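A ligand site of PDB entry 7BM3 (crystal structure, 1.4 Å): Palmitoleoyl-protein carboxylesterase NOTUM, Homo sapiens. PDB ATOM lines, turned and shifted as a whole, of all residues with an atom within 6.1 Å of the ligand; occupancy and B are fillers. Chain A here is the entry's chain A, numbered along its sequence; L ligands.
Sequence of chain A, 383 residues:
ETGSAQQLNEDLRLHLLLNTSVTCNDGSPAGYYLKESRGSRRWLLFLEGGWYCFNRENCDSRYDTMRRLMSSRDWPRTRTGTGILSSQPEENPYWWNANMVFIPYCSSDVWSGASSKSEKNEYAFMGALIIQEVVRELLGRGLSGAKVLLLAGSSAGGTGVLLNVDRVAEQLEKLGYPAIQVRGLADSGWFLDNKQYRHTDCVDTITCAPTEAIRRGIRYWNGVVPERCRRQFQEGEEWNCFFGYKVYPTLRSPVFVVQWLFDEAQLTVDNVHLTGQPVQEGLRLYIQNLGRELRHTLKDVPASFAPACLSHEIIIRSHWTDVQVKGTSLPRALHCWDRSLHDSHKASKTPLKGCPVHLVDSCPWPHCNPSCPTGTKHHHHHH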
ATOM      1  N   GLY A  49       1.277  26.499  13.733  1.00  0.00           N
ATOM      2  CA  GLY A  49       2.503  26.895  13.068  1.00  0.00           C
ATOM      3  C   GLY A  49       2.353  28.160  12.235  1.00  0.00           C
ATOM      4  O   GLY A  49       1.363  28.898  12.328  1.00  0.00           O
ATOM      5  N   GLY A  50       3.382  28.428  11.407  1.00  0.00           N
ATOM      6  CA  GLY A  50       3.386  29.598  10.522  1.00  0.00           C
ATOM      7  C   GLY A  50       4.688  30.375  10.388  1.00  0.00           C
ATOM      8  O   GLY A  50       4.691  31.599  10.510  1.00  0.00           O
ATOM      9  N   TRP A  51       5.780  29.684  10.088  1.00  0.00           N
ATOM     10  CA  TRP A  51       7.084  30.335   9.829  1.00  0.00           C
ATOM     11  C   TRP A  51       7.566  31.043  11.102  1.00  0.00           C
ATOM     12  O   TRP A  51       7.246  30.610  12.209  1.00  0.00           O
ATOM     13  CB  TRP A  51       7.016  31.232   8.589  1.00  0.00           C
ATOM     14  CG  TRP A  51       6.954  30.569   7.261  1.00  0.00           C
ATOM     15  CD1 TRP A  51       5.907  30.596   6.382  1.00  0.00           C
ATOM     16  CD2 TRP A  51       7.986  29.818   6.625  1.00  0.00           C
ATOM     17  NE1 TRP A  51       6.225  29.892   5.241  1.00  0.00           N
ATOM     18  CE2 TRP A  51       7.496  29.400   5.377  1.00  0.00           C
ATOM     19  CE3 TRP A  51       9.281  29.432   6.999  1.00  0.00           C
ATOM     20  CZ2 TRP A  51       8.264  28.635   4.485  1.00  0.00           C
ATOM     21  CZ3 TRP A  51      10.037  28.672   6.125  1.00  0.00           C
ATOM     22  CH2 TRP A  51       9.517  28.271   4.886  1.00  0.00           C
ATOM     23  N   TYR A  52       8.348  32.108  10.930  1.00  0.00           N
ATOM     24  CA  TYR A  52       8.926  32.895  12.022  1.00  0.00           C
ATOM     25  C   TYR A  52       9.496  34.171  11.414  1.00  0.00           C
ATOM     26  O   TYR A  52       9.525  34.328  10.193  1.00  0.00           O
ATOM     27  CB  TYR A  52      10.006  32.117  12.796  1.00  0.00           C
ATOM     28  CG  TYR A  52      11.187  31.615  11.975  1.00  0.00           C
ATOM     29  CD1 TYR A  52      12.320  32.409  11.789  1.00  0.00           C
ATOM     30  CD2 TYR A  52      11.186  30.330  11.436  1.00  0.00           C
ATOM     31  CE1 TYR A  52      13.413  31.948  11.070  1.00  0.00           C
ATOM     32  CE2 TYR A  52      12.277  29.870  10.700  1.00  0.00           C
ATOM     33  CZ  TYR A  52      13.376  30.688  10.530  1.00  0.00           C
ATOM     34  OH  TYR A  52      14.470  30.249   9.806  1.00  0.00           O
ATOM     35  N   TYR A 105      -0.525  30.776  17.413  1.00  0.00           N
ATOM     36  CA  TYR A 105       0.886  31.113  17.311  1.00  0.00           C
ATOM     37  C   TYR A 105       0.967  32.616  17.036  1.00  0.00           C
ATOM     38  O   TYR A 105       0.642  33.051  15.927  1.00  0.00           O
ATOM     39  CB  TYR A 105       1.486  30.331  16.140  1.00  0.00           C
ATOM     40  CG  TYR A 105       2.971  30.499  15.819  1.00  0.00           C
ATOM     41  CD1 TYR A 105       3.942  30.592  16.809  1.00  0.00           C
ATOM     42  CD2 TYR A 105       3.396  30.489  14.484  1.00  0.00           C
ATOM     43  CE1 TYR A 105       5.292  30.704  16.482  1.00  0.00           C
ATOM     44  CE2 TYR A 105       4.746  30.602  14.157  1.00  0.00           C
ATOM     45  CZ  TYR A 105       5.689  30.698  15.156  1.00  0.00           C
ATOM     46  OH  TYR A 105       7.040  30.809  14.846  1.00  0.00           O
ATOM     47  N   SER A 154       1.749  21.370  14.558  1.00  0.00           N
ATOM     48  CA  SER A 154       2.090  21.208  13.144  1.00  0.00           C
ATOM     49  C   SER A 154       3.044  22.304  12.671  1.00  0.00           C
ATOM     50  O   SER A 154       2.893  23.481  13.027  1.00  0.00           O
ATOM     51  CB  SER A 154       0.850  21.226  12.237  1.00  0.00           C
ATOM     52  OG  SER A 154      -0.043  20.149  12.532  1.00  0.00           O
ATOM     53  N   SER A 155       4.021  21.904  11.848  1.00  0.00           N
ATOM     54  CA  SER A 155       4.980  22.843  11.191  1.00  0.00           C
ATOM     55  C   SER A 155       5.835  23.524  12.263  1.00  0.00           C
ATOM     56  O   SER A 155       6.461  22.819  13.078  1.00  0.00           O
ATOM     57  CB  SER A 155       4.236  23.767  10.242  1.00  0.00           C
ATOM     58  OG  SER A 155       3.469  23.028   9.299  1.00  0.00           O
ATOM     59  N   ALA A 156       5.897  24.857  12.337  1.00  0.00           N
ATOM     60  CA  ALA A 156       6.637  25.468  13.430  1.00  0.00           C
ATOM     61  C   ALA A 156       6.091  25.016  14.788  1.00  0.00           C
ATOM     62  O   ALA A 156       6.851  24.967  15.771  1.00  0.00           O
ATOM     63  CB  ALA A 156       6.601  27.005  13.303  1.00  0.00           C
ATOM     64  N   GLY A 157       4.804  24.664  14.863  1.00  0.00           N
ATOM     65  CA  GLY A 157       4.266  24.088  16.084  1.00  0.00           C
ATOM     66  C   GLY A 157       4.753  22.668  16.368  1.00  0.00           C
ATOM     67  O   GLY A 157       4.853  22.257  17.534  1.00  0.00           O
ATOM     68  N   SER A 188       5.058  17.374  10.987  1.00  0.00           N
ATOM     69  CA  SER A 188       5.664  18.248   9.972  1.00  0.00           C
ATOM     70  C   SER A 188       6.645  19.261  10.565  1.00  0.00           C
ATOM     71  O   SER A 188       6.775  20.400  10.070  1.00  0.00           O
ATOM     72  CB  SER A 188       4.603  18.949   9.116  1.00  0.00           C
ATOM     73  OG  SER A 188       3.798  17.980   8.445  1.00  0.00           O
ATOM     74  N   PHE A 191      12.997  18.416  10.300  1.00  0.00           N
ATOM     75  CA  PHE A 191      13.710  18.955   9.140  1.00  0.00           C
ATOM     76  C   PHE A 191      15.176  18.576   9.160  1.00  0.00           C
ATOM     77  O   PHE A 191      15.753  18.249  10.195  1.00  0.00           O
ATOM     78  CB  PHE A 191      13.537  20.477   9.045  1.00  0.00           C
ATOM     79  CG  PHE A 191      12.113  20.889   8.821  1.00  0.00           C
ATOM     80  CD1 PHE A 191      11.380  21.476   9.843  1.00  0.00           C
ATOM     81  CD2 PHE A 191      11.476  20.580   7.631  1.00  0.00           C
ATOM     82  CE1 PHE A 191      10.050  21.818   9.643  1.00  0.00           C
ATOM     83  CE2 PHE A 191      10.145  20.900   7.435  1.00  0.00           C
ATOM     84  CZ  PHE A 191       9.441  21.519   8.446  1.00  0.00           C
ATOM     85  N   LEU A 192      15.782  18.623   7.968  1.00  0.00           N
ATOM     86  CA  LEU A 192      17.207  18.355   7.779  1.00  0.00           C
ATOM     87  C   LEU A 192      17.956  19.642   7.432  1.00  0.00           C
ATOM     88  O   LEU A 192      17.483  20.448   6.607  1.00  0.00           O
ATOM     89  CB  LEU A 192      17.424  17.333   6.657  1.00  0.00           C
ATOM     90  CG  LEU A 192      16.702  16.003   6.831  1.00  0.00           C
ATOM     91  CD1 LEU A 192      16.997  15.100   5.649  1.00  0.00           C
ATOM     92  CD2 LEU A 192      17.106  15.319   8.139  1.00  0.00           C
ATOM     93  N   ASP A 193      19.115  19.829   8.074  1.00  0.00           N
ATOM     94  CA  ASP A 193      20.042  20.918   7.759  1.00  0.00           C
ATOM     95  C   ASP A 193      20.986  20.471   6.651  1.00  0.00           C
ATOM     96  O   ASP A 193      22.202  20.334   6.826  1.00  0.00           O
ATOM     97  CB  ASP A 193      20.771  21.402   9.013  1.00  0.00           C
ATOM     98  CG  ASP A 193      21.433  20.274   9.826  1.00  0.00           C
ATOM     99  OD1 ASP A 193      21.082  19.074   9.694  1.00  0.00           O
ATOM    100  OD2 ASP A 193      22.317  20.605  10.653  1.00  0.00           O
ATOM    101  N   PRO A 210      18.842  29.230   5.220  1.00  0.00           N
ATOM    102  CA  PRO A 210      17.829  28.824   6.206  1.00  0.00           C
ATOM    103  C   PRO A 210      18.381  28.505   7.586  1.00  0.00           C
ATOM    104  O   PRO A 210      17.772  28.870   8.597  1.00  0.00           O
ATOM    105  CB  PRO A 210      17.148  27.610   5.545  1.00  0.00           C
ATOM    106  CG  PRO A 210      17.436  27.775   4.075  1.00  0.00           C
ATOM    107  CD  PRO A 210      18.784  28.417   3.992  1.00  0.00           C
ATOM    108  N   THR A 211      19.525  27.813   7.660  1.00  0.00           N
ATOM    109  CA  THR A 211      20.090  27.473   8.961  1.00  0.00           C
ATOM    110  C   THR A 211      20.607  28.724   9.677  1.00  0.00           C
ATOM    111  O   THR A 211      20.498  28.836  10.910  1.00  0.00           O
ATOM    112  CB  THR A 211      21.197  26.438   8.800  1.00  0.00           C
ATOM    113  OG1 THR A 211      20.741  25.389   7.931  1.00  0.00           O
ATOM    114  CG2 THR A 211      21.561  25.847  10.145  1.00  0.00           C
ATOM    115  N   ALA A 213      19.328  31.732   9.421  1.00  0.00           N
ATOM    116  CA  ALA A 213      18.185  32.475   9.913  1.00  0.00           C
ATOM    117  C   ALA A 213      17.774  32.018  11.319  1.00  0.00           C
ATOM    118  O   ALA A 213      17.362  32.843  12.145  1.00  0.00           O
ATOM    119  CB  ALA A 213      17.019  32.363   8.934  1.00  0.00           C
ATOM    120  N   ILE A 214      17.904  30.719  11.618  1.00  0.00           N
ATOM    121  CA  ILE A 214      17.616  30.222  12.961  1.00  0.00           C
ATOM    122  C   ILE A 214      18.633  30.737  13.977  1.00  0.00           C
ATOM    123  O   ILE A 214      18.264  31.147  15.090  1.00  0.00           O
ATOM    124  CB  ILE A 214      17.547  28.683  12.973  1.00  0.00           C
ATOM    125  CG1 ILE A 214      16.331  28.197  12.164  1.00  0.00           C
ATOM    126  CG2 ILE A 214      17.507  28.160  14.413  1.00  0.00           C
ATOM    127  CD1 ILE A 214      15.001  28.608  12.757  1.00  0.00           C
ATOM    128  N   PHE A 243      16.568  21.105  15.244  1.00  0.00           N
ATOM    129  CA  PHE A 243      16.493  20.031  14.255  1.00  0.00           C
ATOM    130  C   PHE A 243      16.132  18.734  14.946  1.00  0.00           C
ATOM    131  O   PHE A 243      16.851  18.267  15.841  1.00  0.00           O
ATOM    132  CB  PHE A 243      17.788  19.953  13.443  1.00  0.00           C
ATOM    133  CG  PHE A 243      17.933  21.119  12.503  1.00  0.00           C
ATOM    134  CD1 PHE A 243      18.462  22.321  12.936  1.00  0.00           C
ATOM    135  CD2 PHE A 243      17.410  21.048  11.223  1.00  0.00           C
ATOM    136  CE1 PHE A 243      18.530  23.415  12.089  1.00  0.00           C
ATOM    137  CE2 PHE A 243      17.472  22.115  10.368  1.00  0.00           C
ATOM    138  CZ  PHE A 243      18.027  23.305  10.799  1.00  0.00           C
ATOM    139  N   ASP A 263       8.610  16.477   2.312  1.00  0.00           N
ATOM    140  CA  ASP A 263       7.812  17.588   2.806  1.00  0.00           C
ATOM    141  C   ASP A 263       8.023  18.834   1.941  1.00  0.00           C
ATOM    142  O   ASP A 263       9.155  19.189   1.605  1.00  0.00           O
ATOM    143  CB  ASP A 263       8.204  17.868   4.260  1.00  0.00           C
ATOM    144  CG  ASP A 263       7.338  18.897   4.909  1.00  0.00           C
ATOM    145  OD1 ASP A 263       6.433  18.518   5.681  1.00  0.00           O
ATOM    146  OD2 ASP A 263       7.550  20.098   4.656  1.00  0.00           O
ATOM    147  N   GLU A 264       6.918  19.501   1.579  1.00  0.00           N
ATOM    148  CA  GLU A 264       7.005  20.677   0.713  1.00  0.00           C
ATOM    149  C   GLU A 264       7.829  21.801   1.342  1.00  0.00           C
ATOM    150  O   GLU A 264       8.529  22.541   0.625  1.00  0.00           O
ATOM    151  CB  GLU A 264       5.610  21.166   0.359  1.00  0.00           C
ATOM    152  CG  GLU A 264       4.921  20.293  -0.680  1.00  0.00           C
ATOM    153  CD  GLU A 264       3.484  20.708  -0.961  1.00  0.00           C
ATOM    154  OE1 GLU A 264       2.876  20.148  -1.891  1.00  0.00           O
ATOM    155  OE2 GLU A 264       2.963  21.587  -0.229  1.00  0.00           O
ATOM    156  N   ALA A 265       7.756  21.974   2.663  1.00  0.00           N
ATOM    157  CA  ALA A 265       8.549  23.022   3.312  1.00  0.00           C
ATOM    158  C   ALA A 265      10.039  22.715   3.249  1.00  0.00           C
ATOM    159  O   ALA A 265      10.856  23.634   3.070  1.00  0.00           O
ATOM    160  CB  ALA A 265       8.091  23.249   4.756  1.00  0.00           C
ATOM    161  N   GLN A 266      10.407  21.444   3.388  1.00  0.00           N
ATOM    162  CA  GLN A 266      11.802  21.038   3.203  1.00  0.00           C
ATOM    163  C   GLN A 266      12.266  21.323   1.781  1.00  0.00           C
ATOM    164  O   GLN A 266      13.362  21.865   1.564  1.00  0.00           O
ATOM    165  CB  GLN A 266      11.940  19.546   3.522  1.00  0.00           C
ATOM    166  CG  GLN A 266      13.372  18.991   3.365  1.00  0.00           C
ATOM    167  CD  GLN A 266      14.287  19.373   4.518  1.00  0.00           C
ATOM    168  OE1 GLN A 266      13.987  19.108   5.692  1.00  0.00           O
ATOM    169  NE2 GLN A 266      15.431  19.978   4.197  1.00  0.00           N
ATOM    170  N   THR A 268      11.064  23.545  -0.285  1.00  0.00           N
ATOM    171  CA  THR A 268      11.148  24.999  -0.466  1.00  0.00           C
ATOM    172  C   THR A 268      12.464  25.557   0.063  1.00  0.00           C
ATOM    173  O   THR A 268      13.145  26.324  -0.645  1.00  0.00           O
ATOM    174  CB  THR A 268       9.946  25.672   0.223  1.00  0.00           C
ATOM    175  OG1 THR A 268       8.748  25.285  -0.453  1.00  0.00           O
ATOM    176  CG2 THR A 268      10.097  27.193   0.176  1.00  0.00           C
ATOM    177  N   VAL A 269      12.838  25.204   1.296  1.00  0.00           N
ATOM    178  CA  VAL A 269      14.107  25.694   1.828  1.00  0.00           C
ATOM    179  C   VAL A 269      15.294  25.148   1.039  1.00  0.00           C
ATOM    180  O   VAL A 269      16.362  25.782   0.992  1.00  0.00           O
ATOM    181  CB  VAL A 269      14.234  25.486   3.372  1.00  0.00           C
ATOM    182  CG1 VAL A 269      13.083  26.138   4.114  1.00  0.00           C
ATOM    183  CG2 VAL A 269      14.360  24.011   3.728  1.00  0.00           C
ATOM    184  N   HIS A 312       2.336  18.736   2.829  1.00  0.00           N
ATOM    185  CA  HIS A 312       2.742  19.463   4.034  1.00  0.00           C
ATOM    186  C   HIS A 312       1.608  19.493   5.046  1.00  0.00           C
ATOM    187  O   HIS A 312       0.467  19.786   4.679  1.00  0.00           O
ATOM    188  CB  HIS A 312       3.177  20.897   3.706  1.00  0.00           C
ATOM    189  CG  HIS A 312       3.686  21.650   4.894  1.00  0.00           C
ATOM    190  ND1 HIS A 312       4.839  21.300   5.552  1.00  0.00           N
ATOM    191  CD2 HIS A 312       3.186  22.728   5.557  1.00  0.00           C
ATOM    192  CE1 HIS A 312       5.039  22.128   6.569  1.00  0.00           C
ATOM    193  NE2 HIS A 312       4.042  23.006   6.585  1.00  0.00           N
HETATM  194  C1  LIG L   1       4.170  25.732   4.172  1.00  0.00           C
HETATM  195  C2  LIG L   1       4.311  25.294   2.858  1.00  0.00           C
HETATM  196  O1  LIG L   1       3.202  24.819   2.141  1.00  0.00           O
HETATM  197  C3  LIG L   1       5.552  25.332   2.237  1.00  0.00           C
HETATM  198  O2  LIG L   1       5.709  24.896   0.915  1.00  0.00           O
HETATM  199  C4  LIG L   1       6.643  25.807   2.926  1.00  0.00           C
HETATM  200  C5  LIG L   1       6.492  26.223   4.240  1.00  0.00           C
HETATM  201  C6  LIG L   1       5.276  26.186   4.876  1.00  0.00           C
HETATM  202  C7  LIG L   1       5.158  26.717   6.318  1.00  0.00           C
HETATM  203  C8  LIG L   1       5.879  26.073   7.507  1.00  0.00           C
HETATM  204  C9  LIG L   1       5.065  26.559   8.726  1.00  0.00           C
HETATM  205  O3  LIG L   1       5.574  26.767   9.865  1.00  0.00           O
HETATM  206  O4  LIG L   1       3.832  26.780   8.551  1.00  0.00           O
HETATM  207  O5  LIG L   1       7.225  26.504   7.579  1.00  0.00           O
HETATM  208  C10 LIG L   1       8.193  25.556   7.995  1.00  0.00           C
HETATM  209  O6  LIG L   1       7.837  24.447   8.264  1.00  0.00           O
HETATM  210  C11 LIG L   1       9.682  25.912   8.127  1.00  0.00           C
HETATM  211  C12 LIG L   1      10.627  25.003   7.875  1.00  0.00           C
HETATM  212  C13 LIG L   1      12.152  25.222   7.978  1.00  0.00           C
HETATM  213  C14 LIG L   1      12.727  26.442   8.317  1.00  0.00           C
HETATM  214  C15 LIG L   1      14.114  26.563   8.405  1.00  0.00           C
HETATM  215  O7  LIG L   1      14.729  27.788   8.736  1.00  0.00           O
HETATM  216  C16 LIG L   1      14.933  25.478   8.161  1.00  0.00           C
HETATM  217  O8  LIG L   1      16.334  25.628   8.262  1.00  0.00           O
HETATM  218  C17 LIG L   1      14.366  24.258   7.827  1.00  0.00           C
HETATM  219  C18 LIG L   1      12.988  24.138   7.744  1.00  0.00           C
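OH of Tyr 52 sits at hydrogen-bond distance from O7 of the ligand, 2.7 Å away.
N of Trp 51 lies within hydrogen-bond range of O3 of the ligand.
The backbone NH (N) of Ala 156 is in hydrogen-bond range of an oxygen (O3) of the ligand, at 3.1 Å.
N of Gly 50 sits at hydrogen-bond distance from O3 of the ligand, 3.2 Å away.
An oxygen (O7) of the ligand lies within hydrogen-bond range of the backbone carbonyl oxygen (O) of Pro 210.
The side-chain hydroxyl of Thr 268 lies within hydrogen-bond range of an oxygen (O2) of the ligand (3.4 Å).
OH of Tyr 105 sits at hydrogen-bond distance from O of Trp 51.
OG of Ser 155 is in hydrogen-bond range of NE2 of His 312.
OG1 of Thr 268 is in hydrogen-bond range of O of Glu 264 (3.0 Å).
The side-chain carboxylate of Asp 263 is in hydrogen-bond range of the backbone NH of Ala 265.
ND1 of His 312 is in hydrogen-bond range of OD2 of Asp 263.
Ser 155 touches the ligand.
Phe 191 touches the ligand (CZ to O6, 3.3 Å).
Thr 211 touches the ligand (N to O8, 3.9 Å).
CG1 of Ile 214 touches O7 of the ligand, at 3.8 Å.
Phe 243 touches the ligand (CZ to O8, 3.8 Å).
Glu 264 touches the ligand.
Ala 265 touches the ligand (CA to C4, 3.4 Å).
CD2 of His 312 touches C1 of the ligand, at 3.5 Å.
Hydrophobic or aromatic side chains that line the ligand: Trp 51, Tyr 52, Ala 156, Phe 191, Pro 210, Ile 214, Phe 243, Ala 265 and His 312.
14 residues have an atom within 4 Å of the ligand: Gly 50, Trp 51, Tyr 52, Ser 155, Ala 156, Phe 191, Pro 210, Thr 211, Ile 214, Phe 243, Glu 264, Ala 265, Thr 268 and His 312.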
